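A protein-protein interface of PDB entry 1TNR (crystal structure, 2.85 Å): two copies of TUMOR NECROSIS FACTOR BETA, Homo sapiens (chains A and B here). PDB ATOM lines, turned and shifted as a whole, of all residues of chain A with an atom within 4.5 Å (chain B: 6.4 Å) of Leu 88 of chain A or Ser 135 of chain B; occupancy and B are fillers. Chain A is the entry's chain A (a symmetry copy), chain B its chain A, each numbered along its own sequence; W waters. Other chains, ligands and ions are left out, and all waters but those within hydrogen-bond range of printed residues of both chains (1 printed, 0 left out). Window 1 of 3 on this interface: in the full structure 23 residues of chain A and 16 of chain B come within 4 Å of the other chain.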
ATOM      1  N   VAL A  48     -20.482 -12.456 -32.173  1.00  0.00           N
ATOM      2  CA  VAL A  48     -19.814 -13.017 -31.003  1.00  0.00           C
ATOM      3  C   VAL A  48     -20.834 -13.780 -30.176  1.00  0.00           C
ATOM      4  O   VAL A  48     -21.934 -13.278 -29.935  1.00  0.00           O
ATOM      5  CB  VAL A  48     -19.236 -11.896 -30.177  1.00  0.00           C
ATOM      6  CG1 VAL A  48     -18.576 -12.434 -28.964  1.00  0.00           C
ATOM      7  CG2 VAL A  48     -18.257 -11.143 -31.014  1.00  0.00           C
ATOM      8  N   HIS A  72     -23.184 -14.506 -16.854  1.00  0.00           N
ATOM      9  CA  HIS A  72     -22.128 -14.746 -17.799  1.00  0.00           C
ATOM     10  C   HIS A  72     -22.190 -13.508 -18.647  1.00  0.00           C
ATOM     11  O   HIS A  72     -23.273 -12.997 -18.936  1.00  0.00           O
ATOM     12  CB  HIS A  72     -22.393 -15.996 -18.620  1.00  0.00           C
ATOM     13  CG  HIS A  72     -21.234 -16.413 -19.463  1.00  0.00           C
ATOM     14  ND1 HIS A  72     -19.940 -16.455 -18.979  1.00  0.00           N
ATOM     15  CD2 HIS A  72     -21.162 -16.826 -20.754  1.00  0.00           C
ATOM     16  CE1 HIS A  72     -19.123 -16.877 -19.930  1.00  0.00           C
ATOM     17  NE2 HIS A  72     -19.840 -17.115 -21.019  1.00  0.00           N
ATOM     18  N   GLU A  73     -21.041 -13.079 -19.128  1.00  0.00           N
ATOM     19  CA  GLU A  73     -20.979 -11.843 -19.860  1.00  0.00           C
ATOM     20  C   GLU A  73     -19.738 -11.786 -20.770  1.00  0.00           C
ATOM     21  O   GLU A  73     -18.677 -12.326 -20.410  1.00  0.00           O
ATOM     22  CB  GLU A  73     -20.883 -10.801 -18.769  1.00  0.00           C
ATOM     23  CG  GLU A  73     -20.972  -9.378 -19.136  1.00  0.00           C
ATOM     24  CD  GLU A  73     -20.989  -8.547 -17.881  1.00  0.00           C
ATOM     25  OE1 GLU A  73     -22.089  -8.359 -17.306  1.00  0.00           O
ATOM     26  OE2 GLU A  73     -19.895  -8.149 -17.433  1.00  0.00           O
ATOM     27  N   VAL A  74     -19.884 -11.195 -21.960  1.00  0.00           N
ATOM     28  CA  VAL A  74     -18.762 -11.039 -22.889  1.00  0.00           C
ATOM     29  C   VAL A  74     -18.374  -9.573 -22.893  1.00  0.00           C
ATOM     30  O   VAL A  74     -19.216  -8.712 -23.164  1.00  0.00           O
ATOM     31  CB  VAL A  74     -19.119 -11.430 -24.324  1.00  0.00           C
ATOM     32  CG1 VAL A  74     -18.029 -10.976 -25.260  1.00  0.00           C
ATOM     33  CG2 VAL A  74     -19.278 -12.918 -24.439  1.00  0.00           C
ATOM     34  N   PRO A  86     -19.035  -4.325 -21.298  1.00  0.00           N
ATOM     35  CA  PRO A  86     -19.923  -5.461 -21.530  1.00  0.00           C
ATOM     36  C   PRO A  86     -20.631  -5.313 -22.852  1.00  0.00           C
ATOM     37  O   PRO A  86     -21.185  -4.252 -23.127  1.00  0.00           O
ATOM     38  CB  PRO A  86     -20.941  -5.339 -20.385  1.00  0.00           C
ATOM     39  CG  PRO A  86     -20.189  -4.592 -19.341  1.00  0.00           C
ATOM     40  CD  PRO A  86     -19.506  -3.534 -20.161  1.00  0.00           C
ATOM     41  N   LEU A  87     -20.603  -6.371 -23.659  1.00  0.00           N
ATOM     42  CA  LEU A  87     -21.285  -6.398 -24.949  1.00  0.00           C
ATOM     43  C   LEU A  87     -22.570  -7.234 -24.812  1.00  0.00           C
ATOM     44  O   LEU A  87     -23.608  -6.895 -25.377  1.00  0.00           O
ATOM     45  CB  LEU A  87     -20.380  -7.013 -26.016  1.00  0.00           C
ATOM     46  CG  LEU A  87     -19.042  -6.332 -26.300  1.00  0.00           C
ATOM     47  CD1 LEU A  87     -18.148  -7.296 -27.032  1.00  0.00           C
ATOM     48  CD2 LEU A  87     -19.225  -5.062 -27.108  1.00  0.00           C
ATOM     49  N   LEU A  88     -22.498  -8.290 -24.000  1.00  0.00           N
ATOM     50  CA  LEU A  88     -23.611  -9.194 -23.787  1.00  0.00           C
ATOM     51  C   LEU A  88     -23.542  -9.684 -22.333  1.00  0.00           C
ATOM     52  O   LEU A  88     -22.441  -9.994 -21.848  1.00  0.00           O
ATOM     53  CB  LEU A  88     -23.435 -10.406 -24.713  1.00  0.00           C
ATOM     54  CG  LEU A  88     -23.243 -10.153 -26.206  1.00  0.00           C
ATOM     55  CD1 LEU A  88     -22.575 -11.341 -26.855  1.00  0.00           C
ATOM     56  CD2 LEU A  88     -24.580  -9.839 -26.846  1.00  0.00           C
ATOM     57  N   SER A  89     -24.693  -9.761 -21.654  1.00  0.00           N
ATOM     58  CA  SER A  89     -24.784 -10.265 -20.273  1.00  0.00           C
ATOM     59  C   SER A  89     -26.066 -11.053 -20.118  1.00  0.00           C
ATOM     60  O   SER A  89     -27.114 -10.622 -20.603  1.00  0.00           O
ATOM     61  CB  SER A  89     -24.882  -9.142 -19.250  1.00  0.00           C
ATOM     62  OG  SER A  89     -24.372  -7.936 -19.786  1.00  0.00           O
ATOM     63  N   HIS A 108     -26.128 -16.386 -25.430  1.00  0.00           N
ATOM     64  CA  HIS A 108     -26.230 -15.041 -26.011  1.00  0.00           C
ATOM     65  C   HIS A 108     -25.277 -14.813 -27.207  1.00  0.00           C
ATOM     66  O   HIS A 108     -24.212 -15.449 -27.291  1.00  0.00           O
ATOM     67  CB  HIS A 108     -26.088 -13.948 -24.938  1.00  0.00           C
ATOM     68  CG  HIS A 108     -24.796 -13.990 -24.179  1.00  0.00           C
ATOM     69  ND1 HIS A 108     -24.718 -13.730 -22.825  1.00  0.00           N
ATOM     70  CD2 HIS A 108     -23.526 -14.229 -24.588  1.00  0.00           C
ATOM     71  CE1 HIS A 108     -23.458 -13.806 -22.436  1.00  0.00           C
ATOM     72  NE2 HIS A 108     -22.712 -14.106 -23.489  1.00  0.00           N
ATOM     73  N   GLY A 109     -25.698 -13.962 -28.150  1.00  0.00           N
ATOM     74  CA  GLY A 109     -24.885 -13.663 -29.316  1.00  0.00           C
ATOM     75  C   GLY A 109     -25.404 -12.433 -30.045  1.00  0.00           C
ATOM     76  O   GLY A 109     -26.618 -12.193 -30.103  1.00  0.00           O
ATOM     77  N   ALA A 110     -24.490 -11.638 -30.588  1.00  0.00           N
ATOM     78  CA  ALA A 110     -24.869 -10.439 -31.307  1.00  0.00           C
ATOM     79  C   ALA A 110     -23.731 -10.053 -32.228  1.00  0.00           C
ATOM     80  O   ALA A 110     -22.623 -10.617 -32.148  1.00  0.00           O
ATOM     81  CB  ALA A 110     -25.157  -9.324 -30.334  1.00  0.00           C
ATOM     82  N   PHE A 112     -21.133  -7.055 -33.813  1.00  0.00           N
ATOM     83  CA  PHE A 112     -20.523  -5.780 -33.448  1.00  0.00           C
ATOM     84  C   PHE A 112     -19.465  -5.355 -34.433  1.00  0.00           C
ATOM     85  O   PHE A 112     -18.955  -6.166 -35.218  1.00  0.00           O
ATOM     86  CB  PHE A 112     -19.882  -5.859 -32.062  1.00  0.00           C
ATOM     87  CG  PHE A 112     -20.813  -6.364 -30.978  1.00  0.00           C
ATOM     88  CD1 PHE A 112     -21.662  -5.481 -30.295  1.00  0.00           C
ATOM     89  CD2 PHE A 112     -20.835  -7.727 -30.632  1.00  0.00           C
ATOM     90  CE1 PHE A 112     -22.515  -5.952 -29.282  1.00  0.00           C
ATOM     91  CE2 PHE A 112     -21.683  -8.208 -29.621  1.00  0.00           C
ATOM     92  CZ  PHE A 112     -22.526  -7.324 -28.943  1.00  0.00           C
ATOM     93  N   HIS B   5     -27.556  -3.489 -35.310  1.00  0.00           N
ATOM     94  CA  HIS B   5     -27.547  -3.928 -33.940  1.00  0.00           C
ATOM     95  C   HIS B   5     -28.169  -2.794 -33.162  1.00  0.00           C
ATOM     96  O   HIS B   5     -27.628  -1.688 -33.159  1.00  0.00           O
ATOM     97  CB  HIS B   5     -26.141  -4.136 -33.412  1.00  0.00           C
ATOM     98  CG  HIS B   5     -26.147  -4.720 -32.041  1.00  0.00           C
ATOM     99  ND1 HIS B   5     -26.866  -5.861 -31.736  1.00  0.00           N
ATOM    100  CD2 HIS B   5     -25.623  -4.285 -30.874  1.00  0.00           C
ATOM    101  CE1 HIS B   5     -26.784  -6.103 -30.443  1.00  0.00           C
ATOM    102  NE2 HIS B   5     -26.039  -5.163 -29.893  1.00  0.00           N
ATOM    103  N   ILE B   7     -30.121  -1.332 -29.385  1.00  0.00           N
ATOM    104  CA  ILE B   7     -30.321  -1.537 -27.947  1.00  0.00           C
ATOM    105  C   ILE B   7     -31.637  -0.907 -27.458  1.00  0.00           C
ATOM    106  O   ILE B   7     -32.160   0.024 -28.088  1.00  0.00           O
ATOM    107  CB  ILE B   7     -29.165  -0.971 -27.131  1.00  0.00           C
ATOM    108  CG1 ILE B   7     -29.258   0.549 -27.075  1.00  0.00           C
ATOM    109  CG2 ILE B   7     -27.844  -1.416 -27.733  1.00  0.00           C
ATOM    110  CD1 ILE B   7     -28.063   1.203 -26.429  1.00  0.00           C
ATOM    111  N   GLN B  51     -32.562 -10.315 -27.603  1.00  0.00           N
ATOM    112  CA  GLN B  51     -32.480 -10.788 -26.237  1.00  0.00           C
ATOM    113  C   GLN B  51     -33.168  -9.818 -25.300  1.00  0.00           C
ATOM    114  O   GLN B  51     -33.140  -8.619 -25.520  1.00  0.00           O
ATOM    115  CB  GLN B  51     -31.038 -10.957 -25.738  1.00  0.00           C
ATOM    116  CG  GLN B  51     -31.066 -11.445 -24.283  1.00  0.00           C
ATOM    117  CD  GLN B  51     -29.733 -11.545 -23.615  1.00  0.00           C
ATOM    118  OE1 GLN B  51     -29.183 -12.637 -23.464  1.00  0.00           O
ATOM    119  NE2 GLN B  51     -29.237 -10.426 -23.122  1.00  0.00           N
ATOM    120  N   VAL B  53     -34.045  -9.360 -20.851  1.00  0.00           N
ATOM    121  CA  VAL B  53     -33.785  -9.827 -19.492  1.00  0.00           C
ATOM    122  C   VAL B  53     -34.851  -9.148 -18.623  1.00  0.00           C
ATOM    123  O   VAL B  53     -35.119  -7.956 -18.790  1.00  0.00           O
ATOM    124  CB  VAL B  53     -32.377  -9.424 -19.001  1.00  0.00           C
ATOM    125  CG1 VAL B  53     -32.216  -9.821 -17.570  1.00  0.00           C
ATOM    126  CG2 VAL B  53     -31.314 -10.073 -19.845  1.00  0.00           C
ATOM    127  N   TYR B 107     -33.186 -15.567 -25.081  1.00  0.00           N
ATOM    128  CA  TYR B 107     -32.503 -15.224 -26.325  1.00  0.00           C
ATOM    129  C   TYR B 107     -32.982 -16.080 -27.466  1.00  0.00           C
ATOM    130  O   TYR B 107     -33.315 -17.257 -27.256  1.00  0.00           O
ATOM    131  CB  TYR B 107     -31.014 -15.471 -26.194  1.00  0.00           C
ATOM    132  CG  TYR B 107     -30.267 -15.095 -27.445  1.00  0.00           C
ATOM    133  CD1 TYR B 107     -29.776 -13.811 -27.609  1.00  0.00           C
ATOM    134  CD2 TYR B 107     -30.034 -16.025 -28.463  1.00  0.00           C
ATOM    135  CE1 TYR B 107     -29.062 -13.454 -28.754  1.00  0.00           C
ATOM    136  CE2 TYR B 107     -29.331 -15.677 -29.605  1.00  0.00           C
ATOM    137  CZ  TYR B 107     -28.849 -14.386 -29.737  1.00  0.00           C
ATOM    138  OH  TYR B 107     -28.119 -14.019 -30.829  1.00  0.00           O
ATOM    139  N   SER B 133     -30.467  -2.262 -20.391  1.00  0.00           N
ATOM    140  CA  SER B 133     -29.064  -1.929 -20.464  1.00  0.00           C
ATOM    141  C   SER B 133     -28.637  -2.386 -21.859  1.00  0.00           C
ATOM    142  O   SER B 133     -29.310  -3.233 -22.490  1.00  0.00           O
ATOM    143  CB  SER B 133     -28.250  -2.611 -19.356  1.00  0.00           C
ATOM    144  OG  SER B 133     -27.853  -3.933 -19.680  1.00  0.00           O
ATOM    145  N   PRO B 134     -27.576  -1.783 -22.407  1.00  0.00           N
ATOM    146  CA  PRO B 134     -27.150  -2.195 -23.744  1.00  0.00           C
ATOM    147  C   PRO B 134     -26.661  -3.644 -23.844  1.00  0.00           C
ATOM    148  O   PRO B 134     -26.659  -4.208 -24.930  1.00  0.00           O
ATOM    149  CB  PRO B 134     -26.060  -1.171 -24.108  1.00  0.00           C
ATOM    150  CG  PRO B 134     -25.496  -0.784 -22.763  1.00  0.00           C
ATOM    151  CD  PRO B 134     -26.761  -0.637 -21.931  1.00  0.00           C
ATOM    152  N   SER B 135     -26.254  -4.255 -22.738  1.00  0.00           N
ATOM    153  CA  SER B 135     -25.793  -5.628 -22.843  1.00  0.00           C
ATOM    154  C   SER B 135     -26.881  -6.652 -22.570  1.00  0.00           C
ATOM    155  O   SER B 135     -26.684  -7.835 -22.885  1.00  0.00           O
ATOM    156  CB  SER B 135     -24.586  -5.872 -21.949  1.00  0.00           C
ATOM    157  OG  SER B 135     -24.793  -5.351 -20.656  1.00  0.00           O
ATOM    158  N   THR B 136     -28.043  -6.199 -22.086  1.00  0.00           N
ATOM    159  CA  THR B 136     -29.134  -7.114 -21.764  1.00  0.00           C
ATOM    160  C   THR B 136     -30.340  -7.121 -22.686  1.00  0.00           C
ATOM    161  O   THR B 136     -30.996  -8.163 -22.845  1.00  0.00           O
ATOM    162  CB  THR B 136     -29.674  -6.858 -20.360  1.00  0.00           C
ATOM    163  OG1 THR B 136     -30.065  -5.485 -20.246  1.00  0.00           O
ATOM    164  CG2 THR B 136     -28.621  -7.157 -19.343  1.00  0.00           C
ATOM    165  N   VAL B 137     -30.696  -5.957 -23.213  1.00  0.00           N
ATOM    166  CA  VAL B 137     -31.849  -5.862 -24.092  1.00  0.00           C
ATOM    167  C   VAL B 137     -31.444  -5.290 -25.472  1.00  0.00           C
ATOM    168  O   VAL B 137     -31.212  -4.079 -25.622  1.00  0.00           O
ATOM    169  CB  VAL B 137     -32.942  -5.004 -23.440  1.00  0.00           C
ATOM    170  CG1 VAL B 137     -34.066  -4.802 -24.393  1.00  0.00           C
ATOM    171  CG2 VAL B 137     -33.466  -5.669 -22.197  1.00  0.00           C
ATOM    172  N   PHE B 138     -31.354  -6.171 -26.467  1.00  0.00           N
ATOM    173  CA  PHE B 138     -30.973  -5.786 -27.814  1.00  0.00           C
ATOM    174  C   PHE B 138     -31.727  -6.542 -28.917  1.00  0.00           C
ATOM    175  O   PHE B 138     -32.401  -7.558 -28.668  1.00  0.00           O
ATOM    176  CB  PHE B 138     -29.475  -5.936 -27.998  1.00  0.00           C
ATOM    177  CG  PHE B 138     -28.965  -7.304 -27.695  1.00  0.00           C
ATOM    178  CD1 PHE B 138     -29.021  -8.314 -28.656  1.00  0.00           C
ATOM    179  CD2 PHE B 138     -28.409  -7.588 -26.446  1.00  0.00           C
ATOM    180  CE1 PHE B 138     -28.539  -9.598 -28.373  1.00  0.00           C
ATOM    181  CE2 PHE B 138     -27.922  -8.859 -26.149  1.00  0.00           C
ATOM    182  CZ  PHE B 138     -27.985  -9.869 -27.121  1.00  0.00           C
HETATM  183  O   HOH W   1     -25.082  -5.005 -27.142  1.00  0.00           O
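Pro 86 of chain A touches Ser 135 of chain B.
Ser 135 of chain B touches Leu 87 of chain A (CA to O, 3.6 Å).
Leu 88 of chain A touches Ser 135 of chain B (CA to O, 3.5 Å).
Leu 88 of chain A touches Phe 138 of chain B.
Ser 89 of chain A touches Thr 136 of chain B.
His 108 of chain A touches Gln 51 of chain B (CB to OE1, 3.7 Å).
Phe 138 of chain B touches Gly 109 of chain A.
His 5 of chain B touches Ala 110 of chain A (CE1 to CB, 3.6 Å).
CE1 of Phe 138 of chain B touches CB of Ala 110 of chain A (3.9 Å).
Phe 112 of chain A touches His 5 of chain B.
The side-chain hydroxyl (OG) of Ser 133 of chain B sits close to the backbone NH (N) of Ser 135 of chain B.
OG of Ser 133 of chain B is in hydrogen-bond range of OG1 of Thr 136 of chain B.
The backbone NH (N) of Val 48 of chain A sits at hydrogen-bond distance from the backbone carbonyl oxygen (O) of Ala 110 of chain A, at 2.8 Å.
The side-chain carboxylate of Glu 73 of chain A sits at hydrogen-bond distance from the side-chain hydroxyl of Ser 89 of chain A (3.4 Å).
The backbone NH (N) of Leu 87 of chain A is in hydrogen-bond range of the backbone carbonyl oxygen (O) of Val 74 of chain A (2.8 Å).
The backbone NH (N) of Val 74 of chain A lies within hydrogen-bond range of the backbone carbonyl oxygen (O) of Leu 88 of chain A.
Hydrophobic or aromatic side chains of chain B within 4 Å of the printed part of chain A: His 5, Tyr 107 and Phe 138.
Hydrophobic or aromatic side chains of chain A that line the printed part of chain B: Pro 86, Leu 88, His 108, Ala 110 and Phe 112.
Among the printed residues, 13 pairs touch across the chains.
Among the printed residues, no Asp or Glu carboxylate lies within 4 Å of a Lys or Arg side-chain nitrogen of the other chain.
Of chain B, only Ser 135 (3.5 Å) and Phe 138 (3.4 Å) come within 4 Å of Leu 88 of chain A.
Ser 135 of chain B touches just these residues of chain A: Pro 86, Leu 87, Leu 88 and Ser 89.
Of the printed residues of chain A, Tyr 107 of chain B touches Gly 109.
Of the printed residues of chain B, Phe 112 of chain A touches His 5.
Printed residues of chain A within 4 Å of His 5 of chain B: Ala 110 (3.6 Å) and Phe 112 (3.7 Å).
His 72 of chain A touches none of the printed residues of chain B.
The nearest printed residue of chain A that does not touch Tyr 107 of chain B is His 108 of chain A (4.1 Å).
The backbone carbonyl oxygen (O) of Ser 89 of chain A is in hydrogen-bond range of the side-chain amide nitrogen (NE2) of Gln 51 of chain B (3.3 Å).
The side-chain hydroxyl of Tyr 107 of chain B lies within hydrogen-bond range of the backbone carbonyl oxygen of Gly 109 of chain A (2.5 Å).
The side-chain hydroxyl of Ser 135 of chain B is in hydrogen-bond range of the side-chain hydroxyl of Ser 89 of chain A, 2.8 Å away.
No position is printed for both chains.
Of the 13 pairs that touch across the chains among the printed residues, none has its exchanged pair printed and touching as well.
Water W1 lies within hydrogen-bond range of the backbone carbonyl oxygen of Pro 134 of chain B (2.8 Å), a ring nitrogen (NE2) of His 5 of chain B (2.9 Å) and the backbone carbonyl oxygen of Leu 87 of chain A (3.0 Å).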
